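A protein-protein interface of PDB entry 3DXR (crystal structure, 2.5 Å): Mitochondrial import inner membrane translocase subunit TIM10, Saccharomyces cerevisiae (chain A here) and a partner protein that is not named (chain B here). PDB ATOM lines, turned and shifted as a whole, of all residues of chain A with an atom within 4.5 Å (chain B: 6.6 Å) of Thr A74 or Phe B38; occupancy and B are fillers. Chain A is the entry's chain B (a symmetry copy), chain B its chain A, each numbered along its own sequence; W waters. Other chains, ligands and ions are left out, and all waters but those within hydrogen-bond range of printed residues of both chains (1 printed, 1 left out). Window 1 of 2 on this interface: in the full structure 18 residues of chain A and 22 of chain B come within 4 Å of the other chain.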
ATOM      1  N   ASN A  41     -10.955  22.992   1.862  1.00  0.00           N
ATOM      2  CA  ASN A  41     -12.276  23.443   1.492  1.00  0.00           C
ATOM      3  C   ASN A  41     -13.082  23.839   2.715  1.00  0.00           C
ATOM      4  O   ASN A  41     -13.565  24.978   2.809  1.00  0.00           O
ATOM      5  CB  ASN A  41     -12.991  22.349   0.715  1.00  0.00           C
ATOM      6  CG  ASN A  41     -12.863  22.529  -0.790  1.00  0.00           C
ATOM      7  OD1 ASN A  41     -13.461  23.439  -1.377  1.00  0.00           O
ATOM      8  ND2 ASN A  41     -12.075  21.664  -1.424  1.00  0.00           N
ATOM      9  N   LYS A  45     -14.931  27.327   4.200  1.00  0.00           N
ATOM     10  CA  LYS A  45     -16.373  27.344   4.427  1.00  0.00           C
ATOM     11  C   LYS A  45     -16.757  27.629   5.872  1.00  0.00           C
ATOM     12  O   LYS A  45     -17.762  28.286   6.127  1.00  0.00           O
ATOM     13  CB  LYS A  45     -16.993  25.993   4.050  1.00  0.00           C
ATOM     14  CG  LYS A  45     -16.803  25.576   2.617  1.00  0.00           C
ATOM     15  CD  LYS A  45     -17.748  26.322   1.703  1.00  0.00           C
ATOM     16  CE  LYS A  45     -17.622  25.850   0.268  1.00  0.00           C
ATOM     17  NZ  LYS A  45     -18.655  26.511  -0.562  1.00  0.00           N
ATOM     18  N   CYS A  67     -19.874  20.078   7.161  1.00  0.00           N
ATOM     19  CA  CYS A  67     -19.101  20.367   5.958  1.00  0.00           C
ATOM     20  C   CYS A  67     -18.495  19.086   5.401  1.00  0.00           C
ATOM     21  O   CYS A  67     -18.605  18.806   4.206  1.00  0.00           O
ATOM     22  CB  CYS A  67     -17.979  21.383   6.237  1.00  0.00           C
ATOM     23  SG  CYS A  67     -17.031  21.841   4.734  1.00  0.00           S
ATOM     24  N   LYS A  70     -21.323  16.970   3.875  1.00  0.00           N
ATOM     25  CA  LYS A  70     -21.798  17.402   2.561  1.00  0.00           C
ATOM     26  C   LYS A  70     -20.742  17.200   1.479  1.00  0.00           C
ATOM     27  O   LYS A  70     -21.067  17.083   0.302  1.00  0.00           O
ATOM     28  CB  LYS A  70     -22.231  18.865   2.576  1.00  0.00           C
ATOM     29  CG  LYS A  70     -23.456  19.152   3.401  1.00  0.00           C
ATOM     30  CD  LYS A  70     -24.027  20.503   3.013  1.00  0.00           C
ATOM     31  CE  LYS A  70     -25.354  20.771   3.688  1.00  0.00           C
ATOM     32  NZ  LYS A  70     -26.042  21.920   3.042  1.00  0.00           N
ATOM     33  N   TYR A  71     -19.476  17.163   1.877  1.00  0.00           N
ATOM     34  CA  TYR A  71     -18.397  16.962   0.922  1.00  0.00           C
ATOM     35  C   TYR A  71     -18.443  15.534   0.378  1.00  0.00           C
ATOM     36  O   TYR A  71     -18.177  15.299  -0.795  1.00  0.00           O
ATOM     37  CB  TYR A  71     -17.047  17.211   1.585  1.00  0.00           C
ATOM     38  CG  TYR A  71     -15.937  17.449   0.602  1.00  0.00           C
ATOM     39  CD1 TYR A  71     -15.720  18.720   0.075  1.00  0.00           C
ATOM     40  CD2 TYR A  71     -15.107  16.403   0.185  1.00  0.00           C
ATOM     41  CE1 TYR A  71     -14.709  18.952  -0.840  1.00  0.00           C
ATOM     42  CE2 TYR A  71     -14.087  16.628  -0.738  1.00  0.00           C
ATOM     43  CZ  TYR A  71     -13.897  17.910  -1.246  1.00  0.00           C
ATOM     44  OH  TYR A  71     -12.905  18.161  -2.172  1.00  0.00           O
ATOM     45  N   PHE A  72     -18.761  14.573   1.238  1.00  0.00           N
ATOM     46  CA  PHE A  72     -18.865  13.191   0.785  1.00  0.00           C
ATOM     47  C   PHE A  72     -20.139  13.046  -0.019  1.00  0.00           C
ATOM     48  O   PHE A  72     -20.169  12.372  -1.046  1.00  0.00           O
ATOM     49  CB  PHE A  72     -18.886  12.219   1.966  1.00  0.00           C
ATOM     50  CG  PHE A  72     -17.521  11.849   2.457  1.00  0.00           C
ATOM     51  CD1 PHE A  72     -16.817  12.699   3.300  1.00  0.00           C
ATOM     52  CD2 PHE A  72     -16.919  10.660   2.043  1.00  0.00           C
ATOM     53  CE1 PHE A  72     -15.526  12.372   3.730  1.00  0.00           C
ATOM     54  CE2 PHE A  72     -15.632  10.325   2.465  1.00  0.00           C
ATOM     55  CZ  PHE A  72     -14.934  11.183   3.311  1.00  0.00           C
ATOM     56  N   GLU A  73     -21.198  13.691   0.448  1.00  0.00           N
ATOM     57  CA  GLU A  73     -22.455  13.620  -0.271  1.00  0.00           C
ATOM     58  C   GLU A  73     -22.230  14.199  -1.669  1.00  0.00           C
ATOM     59  O   GLU A  73     -22.792  13.710  -2.644  1.00  0.00           O
ATOM     60  CB  GLU A  73     -23.541  14.394   0.478  1.00  0.00           C
ATOM     61  CG  GLU A  73     -24.951  14.031   0.053  1.00  0.00           C
ATOM     62  CD  GLU A  73     -26.004  14.737   0.882  1.00  0.00           C
ATOM     63  OE1 GLU A  73     -25.634  15.355   1.905  1.00  0.00           O
ATOM     64  OE2 GLU A  73     -27.197  14.670   0.517  1.00  0.00           O
ATOM     65  N   THR A  74     -21.376  15.220  -1.755  1.00  0.00           N
ATOM     66  CA  THR A  74     -21.065  15.862  -3.028  1.00  0.00           C
ATOM     67  C   THR A  74     -20.264  14.913  -3.916  1.00  0.00           C
ATOM     68  O   THR A  74     -20.470  14.886  -5.124  1.00  0.00           O
ATOM     69  CB  THR A  74     -20.308  17.218  -2.804  1.00  0.00           C
ATOM     70  OG1 THR A  74     -21.193  18.145  -2.151  1.00  0.00           O
ATOM     71  CG2 THR A  74     -19.842  17.839  -4.147  1.00  0.00           C
ATOM     72  N   ASN A  75     -19.362  14.135  -3.316  1.00  0.00           N
ATOM     73  CA  ASN A  75     -18.563  13.152  -4.059  1.00  0.00           C
ATOM     74  C   ASN A  75     -19.480  12.232  -4.848  1.00  0.00           C
ATOM     75  O   ASN A  75     -19.431  12.178  -6.075  1.00  0.00           O
ATOM     76  CB  ASN A  75     -17.744  12.259  -3.117  1.00  0.00           C
ATOM     77  CG  ASN A  75     -16.383  12.818  -2.813  1.00  0.00           C
ATOM     78  OD1 ASN A  75     -16.202  13.546  -1.838  1.00  0.00           O
ATOM     79  ND2 ASN A  75     -15.413  12.486  -3.653  1.00  0.00           N
ATOM     80  N   VAL A  76     -20.308  11.496  -4.112  1.00  0.00           N
ATOM     81  CA  VAL A  76     -21.254  10.547  -4.684  1.00  0.00           C
ATOM     82  C   VAL A  76     -22.115  11.240  -5.722  1.00  0.00           C
ATOM     83  O   VAL A  76     -22.291  10.737  -6.828  1.00  0.00           O
ATOM     84  CB  VAL A  76     -22.169   9.945  -3.585  1.00  0.00           C
ATOM     85  CG1 VAL A  76     -23.214   9.045  -4.214  1.00  0.00           C
ATOM     86  CG2 VAL A  76     -21.325   9.161  -2.591  1.00  0.00           C
ATOM     87  N   GLN A  77     -22.649  12.399  -5.356  1.00  0.00           N
ATOM     88  CA  GLN A  77     -23.480  13.173  -6.270  1.00  0.00           C
ATOM     89  C   GLN A  77     -22.730  13.378  -7.591  1.00  0.00           C
ATOM     90  O   GLN A  77     -23.232  13.032  -8.659  1.00  0.00           O
ATOM     91  CB  GLN A  77     -23.813  14.533  -5.654  1.00  0.00           C
ATOM     92  CG  GLN A  77     -24.882  15.293  -6.407  1.00  0.00           C
ATOM     93  CD  GLN A  77     -26.269  14.756  -6.132  1.00  0.00           C
ATOM     94  OE1 GLN A  77     -26.429  13.633  -5.652  1.00  0.00           O
ATOM     95  NE2 GLN A  77     -27.283  15.550  -6.443  1.00  0.00           N
ATOM     96  N   VAL A  78     -21.528  13.942  -7.506  1.00  0.00           N
ATOM     97  CA  VAL A  78     -20.703  14.190  -8.686  1.00  0.00           C
ATOM     98  C   VAL A  78     -20.315  12.871  -9.355  1.00  0.00           C
ATOM     99  O   VAL A  78     -20.083  12.816 -10.559  1.00  0.00           O
ATOM    100  CB  VAL A  78     -19.423  14.973  -8.302  1.00  0.00           C
ATOM    101  CG1 VAL A  78     -18.474  15.073  -9.486  1.00  0.00           C
ATOM    102  CG2 VAL A  78     -19.805  16.358  -7.817  1.00  0.00           C
ATOM    103  N   TYR B  30     -12.108  14.003 -11.589  1.00  0.00           N
ATOM    104  CA  TYR B  30     -13.091  13.673 -10.564  1.00  0.00           C
ATOM    105  C   TYR B  30     -12.899  14.541  -9.325  1.00  0.00           C
ATOM    106  O   TYR B  30     -13.827  15.197  -8.866  1.00  0.00           O
ATOM    107  CB  TYR B  30     -12.965  12.192 -10.186  1.00  0.00           C
ATOM    108  CG  TYR B  30     -13.738  11.800  -8.946  1.00  0.00           C
ATOM    109  CD1 TYR B  30     -15.135  11.736  -8.958  1.00  0.00           C
ATOM    110  CD2 TYR B  30     -13.074  11.518  -7.747  1.00  0.00           C
ATOM    111  CE1 TYR B  30     -15.851  11.400  -7.806  1.00  0.00           C
ATOM    112  CE2 TYR B  30     -13.780  11.184  -6.591  1.00  0.00           C
ATOM    113  CZ  TYR B  30     -15.167  11.128  -6.628  1.00  0.00           C
ATOM    114  OH  TYR B  30     -15.867  10.805  -5.484  1.00  0.00           O
ATOM    115  N   LEU B  33     -13.265  18.222  -9.993  1.00  0.00           N
ATOM    116  CA  LEU B  33     -14.668  18.475 -10.249  1.00  0.00           C
ATOM    117  C   LEU B  33     -15.411  18.558  -8.929  1.00  0.00           C
ATOM    118  O   LEU B  33     -16.204  19.466  -8.701  1.00  0.00           O
ATOM    119  CB  LEU B  33     -15.258  17.361 -11.112  1.00  0.00           C
ATOM    120  CG  LEU B  33     -16.753  17.494 -11.421  1.00  0.00           C
ATOM    121  CD1 LEU B  33     -17.045  18.864 -12.018  1.00  0.00           C
ATOM    122  CD2 LEU B  33     -17.175  16.384 -12.369  1.00  0.00           C
ATOM    123  N   VAL B  34     -15.148  17.598  -8.058  1.00  0.00           N
ATOM    124  CA  VAL B  34     -15.794  17.569  -6.761  1.00  0.00           C
ATOM    125  C   VAL B  34     -15.518  18.889  -6.040  1.00  0.00           C
ATOM    126  O   VAL B  34     -16.436  19.543  -5.547  1.00  0.00           O
ATOM    127  CB  VAL B  34     -15.266  16.386  -5.906  1.00  0.00           C
ATOM    128  CG1 VAL B  34     -15.929  16.385  -4.544  1.00  0.00           C
ATOM    129  CG2 VAL B  34     -15.540  15.066  -6.615  1.00  0.00           C
ATOM    130  N   GLU B  35     -14.246  19.275  -6.005  1.00  0.00           N
ATOM    131  CA  GLU B  35     -13.818  20.501  -5.351  1.00  0.00           C
ATOM    132  C   GLU B  35     -14.405  21.751  -5.995  1.00  0.00           C
ATOM    133  O   GLU B  35     -14.776  22.705  -5.308  1.00  0.00           O
ATOM    134  CB  GLU B  35     -12.292  20.600  -5.366  1.00  0.00           C
ATOM    135  CG  GLU B  35     -11.786  21.858  -4.689  1.00  0.00           C
ATOM    136  CD  GLU B  35     -10.282  21.891  -4.536  1.00  0.00           C
ATOM    137  OE1 GLU B  35      -9.568  22.002  -5.556  1.00  0.00           O
ATOM    138  OE2 GLU B  35      -9.817  21.803  -3.381  1.00  0.00           O
ATOM    139  N   ARG B  36     -14.483  21.745  -7.317  1.00  0.00           N
ATOM    140  CA  ARG B  36     -15.028  22.878  -8.049  1.00  0.00           C
ATOM    141  C   ARG B  36     -16.490  23.105  -7.660  1.00  0.00           C
ATOM    142  O   ARG B  36     -16.886  24.220  -7.298  1.00  0.00           O
ATOM    143  CB  ARG B  36     -14.922  22.616  -9.558  1.00  0.00           C
ATOM    144  CG  ARG B  36     -15.592  23.663 -10.460  1.00  0.00           C
ATOM    145  CD  ARG B  36     -14.954  25.054 -10.366  1.00  0.00           C
ATOM    146  NE  ARG B  36     -14.988  25.611  -9.010  1.00  0.00           N
ATOM    147  CZ  ARG B  36     -14.720  26.881  -8.718  1.00  0.00           C
ATOM    148  NH1 ARG B  36     -14.400  27.731  -9.685  1.00  0.00           N
ATOM    149  NH2 ARG B  36     -14.778  27.307  -7.464  1.00  0.00           N
ATOM    150  N   CYS B  37     -17.277  22.034  -7.713  1.00  0.00           N
ATOM    151  CA  CYS B  37     -18.694  22.112  -7.416  1.00  0.00           C
ATOM    152  C   CYS B  37     -19.039  22.240  -5.938  1.00  0.00           C
ATOM    153  O   CYS B  37     -20.086  22.773  -5.589  1.00  0.00           O
ATOM    154  CB  CYS B  37     -19.421  20.919  -8.043  1.00  0.00           C
ATOM    155  SG  CYS B  37     -19.234  20.849  -9.856  1.00  0.00           S
ATOM    156  N   PHE B  38     -18.173  21.756  -5.065  1.00  0.00           N
ATOM    157  CA  PHE B  38     -18.442  21.901  -3.644  1.00  0.00           C
ATOM    158  C   PHE B  38     -18.246  23.369  -3.271  1.00  0.00           C
ATOM    159  O   PHE B  38     -19.012  23.937  -2.505  1.00  0.00           O
ATOM    160  CB  PHE B  38     -17.487  21.052  -2.817  1.00  0.00           C
ATOM    161  CG  PHE B  38     -17.745  21.135  -1.348  1.00  0.00           C
ATOM    162  CD1 PHE B  38     -18.778  20.406  -0.767  1.00  0.00           C
ATOM    163  CD2 PHE B  38     -16.965  21.957  -0.541  1.00  0.00           C
ATOM    164  CE1 PHE B  38     -19.027  20.492   0.597  1.00  0.00           C
ATOM    165  CE2 PHE B  38     -17.204  22.054   0.820  1.00  0.00           C
ATOM    166  CZ  PHE B  38     -18.239  21.319   1.394  1.00  0.00           C
ATOM    167  N   THR B  39     -17.200  23.970  -3.826  1.00  0.00           N
ATOM    168  CA  THR B  39     -16.869  25.370  -3.580  1.00  0.00           C
ATOM    169  C   THR B  39     -17.962  26.307  -4.100  1.00  0.00           C
ATOM    170  O   THR B  39     -18.352  27.246  -3.400  1.00  0.00           O
ATOM    171  CB  THR B  39     -15.539  25.749  -4.261  1.00  0.00           C
ATOM    172  OG1 THR B  39     -14.501  24.903  -3.766  1.00  0.00           O
ATOM    173  CG2 THR B  39     -15.180  27.208  -3.989  1.00  0.00           C
ATOM    174  N   ASP B  40     -18.470  26.054  -5.309  1.00  0.00           N
ATOM    175  CA  ASP B  40     -19.510  26.924  -5.875  1.00  0.00           C
ATOM    176  C   ASP B  40     -20.947  26.673  -5.457  1.00  0.00           C
ATOM    177  O   ASP B  40     -21.779  27.579  -5.567  1.00  0.00           O
ATOM    178  CB  ASP B  40     -19.504  26.889  -7.404  1.00  0.00           C
ATOM    179  CG  ASP B  40     -18.250  27.474  -8.000  1.00  0.00           C
ATOM    180  OD1 ASP B  40     -17.672  28.405  -7.394  1.00  0.00           O
ATOM    181  OD2 ASP B  40     -17.854  27.006  -9.086  1.00  0.00           O
ATOM    182  N   CYS B  41     -21.248  25.463  -4.985  1.00  0.00           N
ATOM    183  CA  CYS B  41     -22.626  25.107  -4.646  1.00  0.00           C
ATOM    184  C   CYS B  41     -23.036  24.912  -3.202  1.00  0.00           C
ATOM    185  O   CYS B  41     -24.151  25.277  -2.818  1.00  0.00           O
ATOM    186  CB  CYS B  41     -23.016  23.842  -5.397  1.00  0.00           C
ATOM    187  SG  CYS B  41     -23.083  24.006  -7.204  1.00  0.00           S
ATOM    188  N   VAL B  42     -22.155  24.321  -2.407  1.00  0.00           N
ATOM    189  CA  VAL B  42     -22.470  24.040  -1.020  1.00  0.00           C
ATOM    190  C   VAL B  42     -22.032  25.152  -0.102  1.00  0.00           C
ATOM    191  O   VAL B  42     -20.869  25.216   0.270  1.00  0.00           O
ATOM    192  CB  VAL B  42     -21.807  22.718  -0.593  1.00  0.00           C
ATOM    193  CG1 VAL B  42     -22.359  22.265   0.728  1.00  0.00           C
ATOM    194  CG2 VAL B  42     -22.051  21.655  -1.660  1.00  0.00           C
ATOM    195  N   ASN B  43     -22.968  26.022   0.275  1.00  0.00           N
ATOM    196  CA  ASN B  43     -22.653  27.147   1.162  1.00  0.00           C
ATOM    197  C   ASN B  43     -23.453  27.161   2.450  1.00  0.00           C
ATOM    198  O   ASN B  43     -23.253  28.025   3.293  1.00  0.00           O
ATOM    199  CB  ASN B  43     -22.884  28.474   0.438  1.00  0.00           C
ATOM    200  CG  ASN B  43     -24.363  28.794   0.237  1.00  0.00           C
ATOM    201  OD1 ASN B  43     -25.238  27.987   0.549  1.00  0.00           O
ATOM    202  ND2 ASN B  43     -24.644  29.984  -0.292  1.00  0.00           N
ATOM    203  N   PHE B  45     -24.494  25.181   5.874  1.00  0.00           N
ATOM    204  CA  PHE B  45     -24.075  24.111   6.762  1.00  0.00           C
ATOM    205  C   PHE B  45     -24.913  24.071   8.032  1.00  0.00           C
ATOM    206  O   PHE B  45     -24.405  23.827   9.124  1.00  0.00           O
ATOM    207  CB  PHE B  45     -22.586  24.245   7.097  1.00  0.00           C
ATOM    208  CG  PHE B  45     -21.709  24.260   5.885  1.00  0.00           C
ATOM    209  CD1 PHE B  45     -21.324  25.463   5.309  1.00  0.00           C
ATOM    210  CD2 PHE B  45     -21.356  23.077   5.256  1.00  0.00           C
ATOM    211  CE1 PHE B  45     -20.601  25.483   4.129  1.00  0.00           C
ATOM    212  CE2 PHE B  45     -20.631  23.090   4.074  1.00  0.00           C
ATOM    213  CZ  PHE B  45     -20.259  24.290   3.505  1.00  0.00           C
ATOM    214  N   LEU B  50     -27.231  17.623   1.523  1.00  0.00           N
ATOM    215  CA  LEU B  50     -27.441  18.546   0.426  1.00  0.00           C
ATOM    216  C   LEU B  50     -28.917  18.830   0.257  1.00  0.00           C
ATOM    217  O   LEU B  50     -29.728  17.914   0.281  1.00  0.00           O
ATOM    218  CB  LEU B  50     -26.905  17.949  -0.875  1.00  0.00           C
ATOM    219  CG  LEU B  50     -25.429  17.584  -0.883  1.00  0.00           C
ATOM    220  CD1 LEU B  50     -25.084  16.948  -2.213  1.00  0.00           C
ATOM    221  CD2 LEU B  50     -24.594  18.829  -0.635  1.00  0.00           C
ATOM    222  N   ILE B  58     -25.076  21.394  -8.245  1.00  0.00           N
ATOM    223  CA  ILE B  58     -23.987  20.452  -8.508  1.00  0.00           C
ATOM    224  C   ILE B  58     -24.204  19.750  -9.846  1.00  0.00           C
ATOM    225  O   ILE B  58     -23.251  19.341 -10.509  1.00  0.00           O
ATOM    226  CB  ILE B  58     -23.889  19.377  -7.402  1.00  0.00           C
ATOM    227  CG1 ILE B  58     -23.648  20.049  -6.050  1.00  0.00           C
ATOM    228  CG2 ILE B  58     -22.750  18.401  -7.703  1.00  0.00           C
ATOM    229  CD1 ILE B  58     -23.674  19.097  -4.882  1.00  0.00           C
ATOM    230  N   CYS B  61     -23.199  22.499 -12.413  1.00  0.00           N
ATOM    231  CA  CYS B  61     -21.750  22.689 -12.304  1.00  0.00           C
ATOM    232  C   CYS B  61     -21.035  21.501 -12.944  1.00  0.00           C
ATOM    233  O   CYS B  61     -20.106  21.675 -13.728  1.00  0.00           O
ATOM    234  CB  CYS B  61     -21.334  22.834 -10.829  1.00  0.00           C
ATOM    235  SG  CYS B  61     -19.537  22.772 -10.484  1.00  0.00           S
HETATM  236  O   HOH W   1     -16.847  27.852  -1.556  1.00  0.00           O
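The side-chain hydroxyl of Tyr B30 lies within hydrogen-bond range of the side-chain amide nitrogen of Asn A75 (2.5 Å). The side-chain carboxylate of Glu B35 sits at hydrogen-bond distance from the side-chain amide nitrogen of Asn A41 (3.0 Å). The backbone carbonyl oxygen (O) of Phe B38 sits at hydrogen-bond distance from the side-chain amino group (NZ) of Lys A45 (3.2 Å). OD1 of Asn A41 sits at hydrogen-bond distance from OG1 of Thr B39, at 3.0 Å. O of Thr B39 is in hydrogen-bond range of NZ of Lys A45 (2.9 Å). The backbone carbonyl oxygen (O) of Val B42 is in hydrogen-bond range of the side-chain amino group (NZ) of Lys A45, 2.7 Å away. The backbone NH (N) of Leu B50 sits at hydrogen-bond distance from the side-chain carboxylate (OE1) of Glu A73, at 2.8 Å.
Water W1 lies within hydrogen-bond range of the backbone carbonyl oxygen of Thr B39 (2.5 Å) and the side-chain amino group of Lys A45 (2.5 Å).
O of Glu B35 sits at hydrogen-bond distance from OG1 of Thr B39. SG of Cys B41 lies within hydrogen-bond range of N of Ile B58, at 3.4 Å. OG1 of Thr A74 is in hydrogen-bond range of O of Lys A70 (2.7 Å). The side-chain amide oxygen (OD1) of Asn A75 lies close to the backbone carbonyl oxygen (O) of Tyr A71, 2.8 Å away. SG of Cys B37 forms a disulfide with SG of Cys B61 (2.0 Å).
Among the printed residues, pairs that only touch across the chains: Asn A41 with Phe B38, Lys A45 with Phe B45, Cys A67 with Phe B38, Cys A67 with Phe B45, Lys A70 with Phe B38, Lys A70 with Val B42, Lys A70 with Leu B50, Tyr A71 with Phe B38, Thr A74 with Phe B38, Thr A74 with Val B42, Thr A74 with Leu B50, Thr A74 with Ile B58, Asn A75 with Val B34, Gln A77 with Ile B58, Val A78 with Leu B33 and Val A78 with Ile B58.
Of the 12 printed residues of chain A, 10 touch a printed residue of chain B. Printed residues of chain A that touch a printed residue of chain B: Asn A41, Lys A45, Cys A67, Lys A70, Tyr A71, Glu A73, Thr A74, Asn A75, Gln A77 and Val A78. Hydrophobic or aromatic side chains of chain A within 4 Å of the printed part of chain B: Tyr A71 and Val A78. Of the 16 printed residues of chain B, 10 touch a printed residue of chain A. Hydrophobic or aromatic side chains of chain B within 4 Å of the printed part of chain A: Tyr B30, Leu B33, Val B34, Phe B38, Val B42, Phe B45, Leu B50 and Ile B58. Along chain B the printed residues that touch a printed residue of chain A span positions 30 to 58.
Of the printed residues of chain B, Thr A74 touches Phe B38 (3.6 Å), Val B42 (3.6 Å), Leu B50 (3.8 Å) and Ile B58 (3.8 Å). Phe B38 touches just these residues of chain A: Asn A41 (3.9 Å), Lys A45 (3.2 Å), Cys A67 (3.6 Å), Lys A70 (3.8 Å), Tyr A71 (3.5 Å) and Thr A74 (3.6 Å). Of the printed residues of chain B, Lys A45 touches Phe B38, Thr B39, Val B42 and Phe B45. Of the printed residues of chain A, Val B42 touches Lys A45, Lys A70 and Thr A74. The nearest residue of chain B that does not touch Thr A74 is Val B34 (4.1 Å). The nearest printed residue of chain B that does not touch Cys A67 is Val B42 (6.2 Å).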
